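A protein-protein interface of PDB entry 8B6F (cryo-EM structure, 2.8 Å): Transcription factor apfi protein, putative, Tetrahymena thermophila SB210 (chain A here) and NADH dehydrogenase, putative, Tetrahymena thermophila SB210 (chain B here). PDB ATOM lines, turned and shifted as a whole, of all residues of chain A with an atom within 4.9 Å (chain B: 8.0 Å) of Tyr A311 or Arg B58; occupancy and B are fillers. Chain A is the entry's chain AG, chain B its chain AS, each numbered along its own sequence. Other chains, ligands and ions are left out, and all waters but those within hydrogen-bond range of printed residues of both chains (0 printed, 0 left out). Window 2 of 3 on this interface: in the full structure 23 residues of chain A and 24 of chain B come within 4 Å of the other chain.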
ATOM      1  N   ASP A 288     -24.172  11.646  16.672  1.00  0.00           N
ATOM      2  CA  ASP A 288     -24.787  10.885  15.600  1.00  0.00           C
ATOM      3  C   ASP A 288     -26.222  10.517  15.973  1.00  0.00           C
ATOM      4  O   ASP A 288     -26.523  10.272  17.144  1.00  0.00           O
ATOM      5  CB  ASP A 288     -23.989   9.618  15.312  1.00  0.00           C
ATOM      6  CG  ASP A 288     -22.632   9.909  14.711  1.00  0.00           C
ATOM      7  OD1 ASP A 288     -22.314  11.099  14.510  1.00  0.00           O
ATOM      8  OD2 ASP A 288     -21.881   8.949  14.440  1.00  0.00           O
ATOM      9  N   GLN A 306     -24.618   1.659  10.968  1.00  0.00           N
ATOM     10  CA  GLN A 306     -23.633   2.650  10.563  1.00  0.00           C
ATOM     11  C   GLN A 306     -22.289   1.978  10.309  1.00  0.00           C
ATOM     12  O   GLN A 306     -21.866   1.092  11.056  1.00  0.00           O
ATOM     13  CB  GLN A 306     -23.497   3.728  11.638  1.00  0.00           C
ATOM     14  CG  GLN A 306     -22.479   4.812  11.315  1.00  0.00           C
ATOM     15  CD  GLN A 306     -22.398   5.871  12.397  1.00  0.00           C
ATOM     16  OE1 GLN A 306     -21.313   6.225  12.855  1.00  0.00           O
ATOM     17  NE2 GLN A 306     -23.550   6.391  12.804  1.00  0.00           N
ATOM     18  N   GLN A 307     -21.617   2.403   9.243  1.00  0.00           N
ATOM     19  CA  GLN A 307     -20.381   1.763   8.798  1.00  0.00           C
ATOM     20  C   GLN A 307     -19.220   2.289   9.628  1.00  0.00           C
ATOM     21  O   GLN A 307     -18.710   3.384   9.385  1.00  0.00           O
ATOM     22  CB  GLN A 307     -20.155   2.015   7.312  1.00  0.00           C
ATOM     23  CG  GLN A 307     -21.261   1.473   6.428  1.00  0.00           C
ATOM     24  CD  GLN A 307     -21.416  -0.028   6.549  1.00  0.00           C
ATOM     25  OE1 GLN A 307     -20.447  -0.745   6.798  1.00  0.00           O
ATOM     26  NE2 GLN A 307     -22.640  -0.514   6.381  1.00  0.00           N
ATOM     27  N   TYR A 308     -18.793   1.496  10.611  1.00  0.00           N
ATOM     28  CA  TYR A 308     -17.666   1.878  11.452  1.00  0.00           C
ATOM     29  C   TYR A 308     -16.333   1.682  10.743  1.00  0.00           C
ATOM     30  O   TYR A 308     -15.354   2.356  11.079  1.00  0.00           O
ATOM     31  CB  TYR A 308     -17.688   1.070  12.748  1.00  0.00           C
ATOM     32  CG  TYR A 308     -19.035   1.055  13.428  1.00  0.00           C
ATOM     33  CD1 TYR A 308     -19.809   2.205  13.504  1.00  0.00           C
ATOM     34  CD2 TYR A 308     -19.541  -0.114  13.976  1.00  0.00           C
ATOM     35  CE1 TYR A 308     -21.042   2.194  14.120  1.00  0.00           C
ATOM     36  CE2 TYR A 308     -20.773  -0.136  14.594  1.00  0.00           C
ATOM     37  CZ  TYR A 308     -21.518   1.022  14.664  1.00  0.00           C
ATOM     38  OH  TYR A 308     -22.747   1.005  15.277  1.00  0.00           O
ATOM     39  N   LYS A 309     -16.276   0.774   9.768  1.00  0.00           N
ATOM     40  CA  LYS A 309     -15.039   0.573   9.023  1.00  0.00           C
ATOM     41  C   LYS A 309     -14.656   1.827   8.249  1.00  0.00           C
ATOM     42  O   LYS A 309     -13.470   2.152   8.129  1.00  0.00           O
ATOM     43  CB  LYS A 309     -15.180  -0.623   8.084  1.00  0.00           C
ATOM     44  CG  LYS A 309     -15.372  -1.942   8.813  1.00  0.00           C
ATOM     45  CD  LYS A 309     -15.373  -3.120   7.854  1.00  0.00           C
ATOM     46  CE  LYS A 309     -15.600  -4.432   8.590  1.00  0.00           C
ATOM     47  NZ  LYS A 309     -14.562  -4.688   9.627  1.00  0.00           N
ATOM     48  N   ARG A 310     -15.645   2.544   7.718  1.00  0.00           N
ATOM     49  CA  ARG A 310     -15.351   3.797   7.033  1.00  0.00           C
ATOM     50  C   ARG A 310     -14.750   4.814   7.993  1.00  0.00           C
ATOM     51  O   ARG A 310     -13.813   5.536   7.634  1.00  0.00           O
ATOM     52  CB  ARG A 310     -16.621   4.350   6.385  1.00  0.00           C
ATOM     53  CG  ARG A 310     -17.163   3.486   5.253  1.00  0.00           C
ATOM     54  CD  ARG A 310     -16.139   3.306   4.140  1.00  0.00           C
ATOM     55  NE  ARG A 310     -16.696   2.617   2.983  1.00  0.00           N
ATOM     56  CZ  ARG A 310     -17.305   3.214   1.968  1.00  0.00           C
ATOM     57  NH1 ARG A 310     -17.478   4.526   1.939  1.00  0.00           N
ATOM     58  NH2 ARG A 310     -17.756   2.477   0.958  1.00  0.00           N
ATOM     59  N   TYR A 311     -15.275   4.892   9.217  1.00  0.00           N
ATOM     60  CA  TYR A 311     -14.693   5.797  10.202  1.00  0.00           C
ATOM     61  C   TYR A 311     -13.258   5.407  10.524  1.00  0.00           C
ATOM     62  O   TYR A 311     -12.383   6.273  10.631  1.00  0.00           O
ATOM     63  CB  TYR A 311     -15.542   5.807  11.472  1.00  0.00           C
ATOM     64  CG  TYR A 311     -16.839   6.565  11.330  1.00  0.00           C
ATOM     65  CD1 TYR A 311     -17.979   5.943  10.847  1.00  0.00           C
ATOM     66  CD2 TYR A 311     -16.922   7.904  11.685  1.00  0.00           C
ATOM     67  CE1 TYR A 311     -19.167   6.631  10.716  1.00  0.00           C
ATOM     68  CE2 TYR A 311     -18.105   8.603  11.558  1.00  0.00           C
ATOM     69  CZ  TYR A 311     -19.224   7.960  11.073  1.00  0.00           C
ATOM     70  OH  TYR A 311     -20.406   8.651  10.945  1.00  0.00           O
ATOM     71  N   ASP A 312     -12.995   4.110  10.692  1.00  0.00           N
ATOM     72  CA  ASP A 312     -11.634   3.669  10.977  1.00  0.00           C
ATOM     73  C   ASP A 312     -10.694   4.009   9.828  1.00  0.00           C
ATOM     74  O   ASP A 312      -9.566   4.463  10.052  1.00  0.00           O
ATOM     75  CB  ASP A 312     -11.616   2.167  11.257  1.00  0.00           C
ATOM     76  CG  ASP A 312     -12.374   1.801  12.517  1.00  0.00           C
ATOM     77  OD1 ASP A 312     -12.423   2.633  13.446  1.00  0.00           O
ATOM     78  OD2 ASP A 312     -12.921   0.681  12.580  1.00  0.00           O
ATOM     79  N   GLU A 313     -11.134   3.779   8.590  1.00  0.00           N
ATOM     80  CA  GLU A 313     -10.297   4.088   7.436  1.00  0.00           C
ATOM     81  C   GLU A 313     -10.037   5.585   7.326  1.00  0.00           C
ATOM     82  O   GLU A 313      -8.918   6.009   7.017  1.00  0.00           O
ATOM     83  CB  GLU A 313     -10.953   3.563   6.161  1.00  0.00           C
ATOM     84  CG  GLU A 313     -11.059   2.050   6.112  1.00  0.00           C
ATOM     85  CD  GLU A 313     -11.942   1.566   4.981  1.00  0.00           C
ATOM     86  OE1 GLU A 313     -12.360   2.402   4.154  1.00  0.00           O
ATOM     87  OE2 GLU A 313     -12.220   0.351   4.921  1.00  0.00           O
ATOM     88  N   ALA A 314     -11.064   6.402   7.571  1.00  0.00           N
ATOM     89  CA  ALA A 314     -10.879   7.848   7.528  1.00  0.00           C
ATOM     90  C   ALA A 314      -9.908   8.309   8.605  1.00  0.00           C
ATOM     91  O   ALA A 314      -9.055   9.167   8.355  1.00  0.00           O
ATOM     92  CB  ALA A 314     -12.226   8.551   7.680  1.00  0.00           C
ATOM     93  N   LYS A 315     -10.017   7.746   9.809  1.00  0.00           N
ATOM     94  CA  LYS A 315      -9.079   8.095  10.869  1.00  0.00           C
ATOM     95  C   LYS A 315      -7.654   7.730  10.473  1.00  0.00           C
ATOM     96  O   LYS A 315      -6.723   8.514  10.687  1.00  0.00           O
ATOM     97  CB  LYS A 315      -9.472   7.397  12.170  1.00  0.00           C
ATOM     98  CG  LYS A 315      -8.489   7.619  13.309  1.00  0.00           C
ATOM     99  CD  LYS A 315      -9.017   7.060  14.620  1.00  0.00           C
ATOM    100  CE  LYS A 315      -8.001   7.233  15.738  1.00  0.00           C
ATOM    101  NZ  LYS A 315      -8.523   6.756  17.047  1.00  0.00           N
ATOM    102  N   GLN B  43     -24.358  23.296  12.513  1.00  0.00           N
ATOM    103  CA  GLN B  43     -23.860  21.929  12.565  1.00  0.00           C
ATOM    104  C   GLN B  43     -23.217  21.661  13.919  1.00  0.00           C
ATOM    105  O   GLN B  43     -22.438  22.477  14.419  1.00  0.00           O
ATOM    106  CB  GLN B  43     -22.837  21.707  11.452  1.00  0.00           C
ATOM    107  CG  GLN B  43     -23.384  21.906  10.053  1.00  0.00           C
ATOM    108  CD  GLN B  43     -24.199  20.731   9.575  1.00  0.00           C
ATOM    109  OE1 GLN B  43     -23.886  19.581   9.876  1.00  0.00           O
ATOM    110  NE2 GLN B  43     -25.257  21.012   8.826  1.00  0.00           N
ATOM    111  N   THR B  44     -23.540  20.517  14.510  1.00  0.00           N
ATOM    112  CA  THR B  44     -22.947  20.170  15.790  1.00  0.00           C
ATOM    113  C   THR B  44     -21.428  20.127  15.648  1.00  0.00           C
ATOM    114  O   THR B  44     -20.915  19.641  14.635  1.00  0.00           O
ATOM    115  CB  THR B  44     -23.466  18.819  16.284  1.00  0.00           C
ATOM    116  OG1 THR B  44     -23.220  17.814  15.293  1.00  0.00           O
ATOM    117  CG2 THR B  44     -24.956  18.892  16.570  1.00  0.00           C
ATOM    118  N   ASN B  48     -13.147  15.955  15.083  1.00  0.00           N
ATOM    119  CA  ASN B  48     -12.200  15.163  14.314  1.00  0.00           C
ATOM    120  C   ASN B  48     -12.324  15.482  12.835  1.00  0.00           C
ATOM    121  O   ASN B  48     -13.393  15.862  12.350  1.00  0.00           O
ATOM    122  CB  ASN B  48     -12.427  13.661  14.511  1.00  0.00           C
ATOM    123  CG  ASN B  48     -12.370  13.250  15.960  1.00  0.00           C
ATOM    124  OD1 ASN B  48     -11.635  13.833  16.754  1.00  0.00           O
ATOM    125  ND2 ASN B  48     -13.154  12.241  16.317  1.00  0.00           N
ATOM    126  N   VAL B  50     -12.223  13.166  10.823  1.00  0.00           N
ATOM    127  CA  VAL B  50     -13.123  12.101  10.393  1.00  0.00           C
ATOM    128  C   VAL B  50     -14.553  12.618  10.341  1.00  0.00           C
ATOM    129  O   VAL B  50     -15.263  12.439   9.345  1.00  0.00           O
ATOM    130  CB  VAL B  50     -12.999  10.885  11.328  1.00  0.00           C
ATOM    131  CG1 VAL B  50     -13.932   9.769  10.885  1.00  0.00           C
ATOM    132  CG2 VAL B  50     -11.566  10.393  11.379  1.00  0.00           C
ATOM    133  N   GLN B  51     -14.994  13.282  11.409  1.00  0.00           N
ATOM    134  CA  GLN B  51     -16.344  13.830  11.429  1.00  0.00           C
ATOM    135  C   GLN B  51     -16.507  14.917  10.376  1.00  0.00           C
ATOM    136  O   GLN B  51     -17.554  15.010   9.724  1.00  0.00           O
ATOM    137  CB  GLN B  51     -16.662  14.372  12.819  1.00  0.00           C
ATOM    138  CG  GLN B  51     -16.640  13.307  13.897  1.00  0.00           C
ATOM    139  CD  GLN B  51     -16.826  13.880  15.282  1.00  0.00           C
ATOM    140  OE1 GLN B  51     -16.647  15.077  15.500  1.00  0.00           O
ATOM    141  NE2 GLN B  51     -17.193  13.026  16.228  1.00  0.00           N
ATOM    142  N   ALA B  52     -15.484  15.752  10.201  1.00  0.00           N
ATOM    143  CA  ALA B  52     -15.542  16.789   9.180  1.00  0.00           C
ATOM    144  C   ALA B  52     -15.679  16.184   7.789  1.00  0.00           C
ATOM    145  O   ALA B  52     -16.467  16.665   6.967  1.00  0.00           O
ATOM    146  CB  ALA B  52     -14.294  17.666   9.267  1.00  0.00           C
ATOM    147  N   SER B  53     -14.915  15.127   7.508  1.00  0.00           N
ATOM    148  CA  SER B  53     -15.005  14.468   6.209  1.00  0.00           C
ATOM    149  C   SER B  53     -16.370  13.826   6.006  1.00  0.00           C
ATOM    150  O   SER B  53     -16.925  13.870   4.903  1.00  0.00           O
ATOM    151  CB  SER B  53     -13.900  13.423   6.076  1.00  0.00           C
ATOM    152  OG  SER B  53     -13.918  12.829   4.790  1.00  0.00           O
ATOM    153  N   MET B  54     -16.927  13.228   7.060  1.00  0.00           N
ATOM    154  CA  MET B  54     -18.268  12.660   6.965  1.00  0.00           C
ATOM    155  C   MET B  54     -19.295  13.737   6.647  1.00  0.00           C
ATOM    156  O   MET B  54     -20.197  13.522   5.830  1.00  0.00           O
ATOM    157  CB  MET B  54     -18.627  11.943   8.264  1.00  0.00           C
ATOM    158  CG  MET B  54     -17.794  10.701   8.532  1.00  0.00           C
ATOM    159  SD  MET B  54     -18.029   9.408   7.301  1.00  0.00           S
ATOM    160  CE  MET B  54     -16.861   8.185   7.890  1.00  0.00           C
ATOM    161  N   LYS B  55     -19.178  14.902   7.282  1.00  0.00           N
ATOM    162  CA  LYS B  55     -20.088  15.999   6.975  1.00  0.00           C
ATOM    163  C   LYS B  55     -19.964  16.419   5.518  1.00  0.00           C
ATOM    164  O   LYS B  55     -20.973  16.659   4.846  1.00  0.00           O
ATOM    165  CB  LYS B  55     -19.808  17.186   7.897  1.00  0.00           C
ATOM    166  CG  LYS B  55     -20.181  16.941   9.343  1.00  0.00           C
ATOM    167  CD  LYS B  55     -19.905  18.164  10.198  1.00  0.00           C
ATOM    168  CE  LYS B  55     -20.307  17.920  11.641  1.00  0.00           C
ATOM    169  NZ  LYS B  55     -20.089  19.124  12.480  1.00  0.00           N
ATOM    170  N   THR B  56     -18.735  16.523   5.013  1.00  0.00           N
ATOM    171  CA  THR B  56     -18.545  16.898   3.617  1.00  0.00           C
ATOM    172  C   THR B  56     -19.184  15.878   2.685  1.00  0.00           C
ATOM    173  O   THR B  56     -19.853  16.248   1.713  1.00  0.00           O
ATOM    174  CB  THR B  56     -17.054  17.038   3.313  1.00  0.00           C
ATOM    175  OG1 THR B  56     -16.479  18.034   4.167  1.00  0.00           O
ATOM    176  CG2 THR B  56     -16.833  17.440   1.862  1.00  0.00           C
ATOM    177  N   LEU B  57     -18.986  14.589   2.960  1.00  0.00           N
ATOM    178  CA  LEU B  57     -19.546  13.557   2.095  1.00  0.00           C
ATOM    179  C   LEU B  57     -21.069  13.585   2.121  1.00  0.00           C
ATOM    180  O   LEU B  57     -21.716  13.420   1.081  1.00  0.00           O
ATOM    181  CB  LEU B  57     -19.026  12.186   2.520  1.00  0.00           C
ATOM    182  CG  LEU B  57     -17.531  11.951   2.294  1.00  0.00           C
ATOM    183  CD1 LEU B  57     -17.105  10.630   2.904  1.00  0.00           C
ATOM    184  CD2 LEU B  57     -17.186  11.987   0.814  1.00  0.00           C
ATOM    185  N   ARG B  58     -21.659  13.781   3.299  1.00  0.00           N
ATOM    186  CA  ARG B  58     -23.114  13.834   3.387  1.00  0.00           C
ATOM    187  C   ARG B  58     -23.672  15.058   2.672  1.00  0.00           C
ATOM    188  O   ARG B  58     -24.710  14.972   2.009  1.00  0.00           O
ATOM    189  CB  ARG B  58     -23.546  13.809   4.851  1.00  0.00           C
ATOM    190  CG  ARG B  58     -23.293  12.467   5.512  1.00  0.00           C
ATOM    191  CD  ARG B  58     -23.189  12.577   7.017  1.00  0.00           C
ATOM    192  NE  ARG B  58     -22.797  11.304   7.608  1.00  0.00           N
ATOM    193  CZ  ARG B  58     -22.532  11.122   8.894  1.00  0.00           C
ATOM    194  NH1 ARG B  58     -22.602  12.117   9.763  1.00  0.00           N
ATOM    195  NH2 ARG B  58     -22.187   9.911   9.320  1.00  0.00           N
ATOM    196  N   PHE B  59     -23.011  16.210   2.804  1.00  0.00           N
ATOM    197  CA  PHE B  59     -23.457  17.392   2.076  1.00  0.00           C
ATOM    198  C   PHE B  59     -23.373  17.180   0.572  1.00  0.00           C
ATOM    199  O   PHE B  59     -24.284  17.563  -0.171  1.00  0.00           O
ATOM    200  CB  PHE B  59     -22.631  18.613   2.481  1.00  0.00           C
ATOM    201  CG  PHE B  59     -22.768  19.769   1.533  1.00  0.00           C
ATOM    202  CD1 PHE B  59     -23.941  20.500   1.473  1.00  0.00           C
ATOM    203  CD2 PHE B  59     -21.720  20.126   0.703  1.00  0.00           C
ATOM    204  CE1 PHE B  59     -24.071  21.562   0.599  1.00  0.00           C
ATOM    205  CE2 PHE B  59     -21.841  21.186  -0.172  1.00  0.00           C
ATOM    206  CZ  PHE B  59     -23.020  21.907  -0.224  1.00  0.00           C
ATOM    207  N   TYR B  60     -22.283  16.574   0.101  1.00  0.00           N
ATOM    208  CA  TYR B  60     -22.149  16.307  -1.326  1.00  0.00           C
ATOM    209  C   TYR B  60     -23.202  15.313  -1.794  1.00  0.00           C
ATOM    210  O   TYR B  60     -23.730  15.433  -2.906  1.00  0.00           O
ATOM    211  CB  TYR B  60     -20.742  15.801  -1.637  1.00  0.00           C
ATOM    212  CG  TYR B  60     -20.450  15.705  -3.116  1.00  0.00           C
ATOM    213  CD1 TYR B  60     -20.427  16.836  -3.917  1.00  0.00           C
ATOM    214  CD2 TYR B  60     -20.188  14.487  -3.704  1.00  0.00           C
ATOM    215  CE1 TYR B  60     -20.156  16.748  -5.268  1.00  0.00           C
ATOM    216  CE2 TYR B  60     -19.915  14.384  -5.052  1.00  0.00           C
ATOM    217  CZ  TYR B  60     -19.901  15.518  -5.829  1.00  0.00           C
ATOM    218  OH  TYR B  60     -19.629  15.421  -7.173  1.00  0.00           O
ATOM    219  N   ARG B  61     -23.524  14.325  -0.957  1.00  0.00           N
ATOM    220  CA  ARG B  61     -24.583  13.384  -1.301  1.00  0.00           C
ATOM    221  C   ARG B  61     -25.917  14.099  -1.464  1.00  0.00           C
ATOM    222  O   ARG B  61     -26.658  13.836  -2.417  1.00  0.00           O
ATOM    223  CB  ARG B  61     -24.691  12.298  -0.230  1.00  0.00           C
ATOM    224  CG  ARG B  61     -25.678  11.194  -0.574  1.00  0.00           C
ATOM    225  CD  ARG B  61     -25.900  10.237   0.586  1.00  0.00           C
ATOM    226  NE  ARG B  61     -24.645   9.728   1.129  1.00  0.00           N
ATOM    227  CZ  ARG B  61     -24.297   9.755   2.409  1.00  0.00           C
ATOM    228  NH1 ARG B  61     -25.104  10.238   3.340  1.00  0.00           N
ATOM    229  NH2 ARG B  61     -23.108   9.281   2.767  1.00  0.00           N
ATOM    230  N   LYS B  62     -26.241  15.009  -0.545  1.00  0.00           N
ATOM    231  CA  LYS B  62     -27.484  15.761  -0.665  1.00  0.00           C
ATOM    232  C   LYS B  62     -27.486  16.608  -1.930  1.00  0.00           C
ATOM    233  O   LYS B  62     -28.499  16.685  -2.633  1.00  0.00           O
ATOM    234  CB  LYS B  62     -27.684  16.639   0.570  1.00  0.00           C
ATOM    235  CG  LYS B  62     -29.060  17.280   0.671  1.00  0.00           C
ATOM    236  CD  LYS B  62     -30.151  16.221   0.706  1.00  0.00           C
ATOM    237  CE  LYS B  62     -31.477  16.782   1.178  1.00  0.00           C
ATOM    238  NZ  LYS B  62     -31.931  17.937   0.371  1.00  0.00           N
ATOM    239  N   PHE B  63     -26.360  17.256  -2.230  1.00  0.00           N
ATOM    240  CA  PHE B  63     -26.267  18.067  -3.438  1.00  0.00           C
ATOM    241  C   PHE B  63     -26.479  17.219  -4.686  1.00  0.00           C
ATOM    242  O   PHE B  63     -27.186  17.629  -5.613  1.00  0.00           O
ATOM    243  CB  PHE B  63     -24.909  18.767  -3.490  1.00  0.00           C
ATOM    244  CG  PHE B  63     -24.617  19.424  -4.804  1.00  0.00           C
ATOM    245  CD1 PHE B  63     -25.020  20.724  -5.047  1.00  0.00           C
ATOM    246  CD2 PHE B  63     -23.928  18.745  -5.795  1.00  0.00           C
ATOM    247  CE1 PHE B  63     -24.751  21.331  -6.254  1.00  0.00           C
ATOM    248  CE2 PHE B  63     -23.654  19.347  -7.005  1.00  0.00           C
ATOM    249  CZ  PHE B  63     -24.065  20.642  -7.235  1.00  0.00           C
ATOM    250  N   CYS B  64     -25.872  16.032  -4.727  1.00  0.00           N
ATOM    251  CA  CYS B  64     -26.048  15.145  -5.872  1.00  0.00           C
ATOM    252  C   CYS B  64     -27.488  14.664  -5.987  1.00  0.00           C
ATOM    253  O   CYS B  64     -28.023  14.548  -7.094  1.00  0.00           O
ATOM    254  CB  CYS B  64     -25.096  13.954  -5.763  1.00  0.00           C
ATOM    255  SG  CYS B  64     -23.355  14.374  -5.981  1.00  0.00           S
ATOM    256  N   ARG B  65     -28.135  14.374  -4.858  1.00  0.00           N
ATOM    257  CA  ARG B  65     -29.531  13.953  -4.903  1.00  0.00           C
ATOM    258  C   ARG B  65     -30.449  15.071  -5.375  1.00  0.00           C
ATOM    259  O   ARG B  65     -31.512  14.798  -5.941  1.00  0.00           O
ATOM    260  CB  ARG B  65     -29.967  13.463  -3.523  1.00  0.00           C
ATOM    261  CG  ARG B  65     -29.482  12.067  -3.189  1.00  0.00           C
ATOM    262  CD  ARG B  65     -29.636  11.766  -1.710  1.00  0.00           C
ATOM    263  NE  ARG B  65     -29.402  10.357  -1.417  1.00  0.00           N
ATOM    264  CZ  ARG B  65     -29.248   9.862  -0.198  1.00  0.00           C
ATOM    265  NH1 ARG B  65     -29.269  10.639   0.872  1.00  0.00           N
ATOM    266  NH2 ARG B  65     -29.071   8.553  -0.047  1.00  0.00           N
ATOM    267  N   ILE B 109     -19.642  23.837   5.509  1.00  0.00           N
ATOM    268  CA  ILE B 109     -20.795  22.973   5.272  1.00  0.00           C
ATOM    269  C   ILE B 109     -22.090  23.730   5.526  1.00  0.00           C
ATOM    270  O   ILE B 109     -23.068  23.578   4.784  1.00  0.00           O
ATOM    271  CB  ILE B 109     -20.699  21.701   6.137  1.00  0.00           C
ATOM    272  CG1 ILE B 109     -19.488  20.861   5.722  1.00  0.00           C
ATOM    273  CG2 ILE B 109     -21.983  20.879   6.041  1.00  0.00           C
ATOM    274  CD1 ILE B 109     -19.552  20.304   4.317  1.00  0.00           C
ATOM    275  N   TYR B 113     -24.970  24.194   2.662  1.00  0.00           N
ATOM    276  CA  TYR B 113     -26.379  23.863   2.835  1.00  0.00           C
ATOM    277  C   TYR B 113     -27.260  25.076   2.580  1.00  0.00           C
ATOM    278  O   TYR B 113     -28.323  24.962   1.962  1.00  0.00           O
ATOM    279  CB  TYR B 113     -26.621  23.320   4.243  1.00  0.00           C
ATOM    280  CG  TYR B 113     -26.341  21.843   4.404  1.00  0.00           C
ATOM    281  CD1 TYR B 113     -26.831  20.914   3.495  1.00  0.00           C
ATOM    282  CD2 TYR B 113     -25.588  21.379   5.472  1.00  0.00           C
ATOM    283  CE1 TYR B 113     -26.578  19.566   3.647  1.00  0.00           C
ATOM    284  CE2 TYR B 113     -25.330  20.035   5.633  1.00  0.00           C
ATOM    285  CZ  TYR B 113     -25.827  19.135   4.718  1.00  0.00           C
ATOM    286  OH  TYR B 113     -25.568  17.795   4.878  1.00  0.00           O
ATOM    287  N   LEU B 116     -27.431  25.660  -1.145  1.00  0.00           N
ATOM    288  CA  LEU B 116     -28.249  24.617  -1.748  1.00  0.00           C
ATOM    289  C   LEU B 116     -29.729  24.894  -1.526  1.00  0.00           C
ATOM    290  O   LEU B 116     -30.541  24.741  -2.444  1.00  0.00           O
ATOM    291  CB  LEU B 116     -27.858  23.257  -1.173  1.00  0.00           C
ATOM    292  CG  LEU B 116     -28.543  22.033  -1.779  1.00  0.00           C
ATOM    293  CD1 LEU B 116     -28.241  21.909  -3.265  1.00  0.00           C
ATOM    294  CD2 LEU B 116     -28.099  20.788  -1.038  1.00  0.00           C
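C of Arg A310 touches CE of Met B54, at 3.98 Å.
Tyr A311 touches Val B50.
CE2 of Tyr A311 touches CG of Met B54 (3.7 Å).
Ala A314 touches Val B50.
Lys A315 touches Val B50 (CA to CG2, 3.4 Å).
Of the 22 printed residues of chain B, 3 touch a printed residue of chain A.
Hydrophobic or aromatic side chains of chain B that line the printed part of chain A: Val B50 and Met B54.
Of the 11 printed residues of chain A, 4 touch a printed residue of chain B.
Hydrophobic or aromatic side chains of chain A that line the printed part of chain B: Tyr A311 and Ala A314.
Along chain A the printed residues that touch a printed residue of chain B span positions 310 to 315.
The side-chain hydroxyl of Tyr A311 lies close to the side-chain amide oxygen of Gln A306, 3.2 Å away.
Of the printed residues of chain B, Arg A310 touches Met B54.
Printed residues of chain B within 4 Å of Tyr A311: Val B50, Met B54 and Arg B58.
Of the printed residues of chain B, Ala A314 touches Val B50 (3.8 Å).
Printed residues of chain B within 4 Å of Lys A315: Val B50 (3.4 Å).
Gln B43 touches none of the printed residues of chain A.
Printed residues of chain A within 4 Å of Val B50: Tyr A311 (3.6 Å), Ala A314 (3.8 Å) and Lys A315 (3.4 Å).
Printed residues of chain A within 4 Å of Met B54: Arg A310 (3.98 Å) and Tyr A311 (3.7 Å).
Printed residues of chain A within 4 Å of Arg B58: Tyr A311 (2.7 Å).
The nearest residue of chain B that does not touch Tyr A311 is Gln B51 (5.5 Å).
OH of Tyr A311 lies within hydrogen-bond range of NH2 of Arg B58 (2.7 Å).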
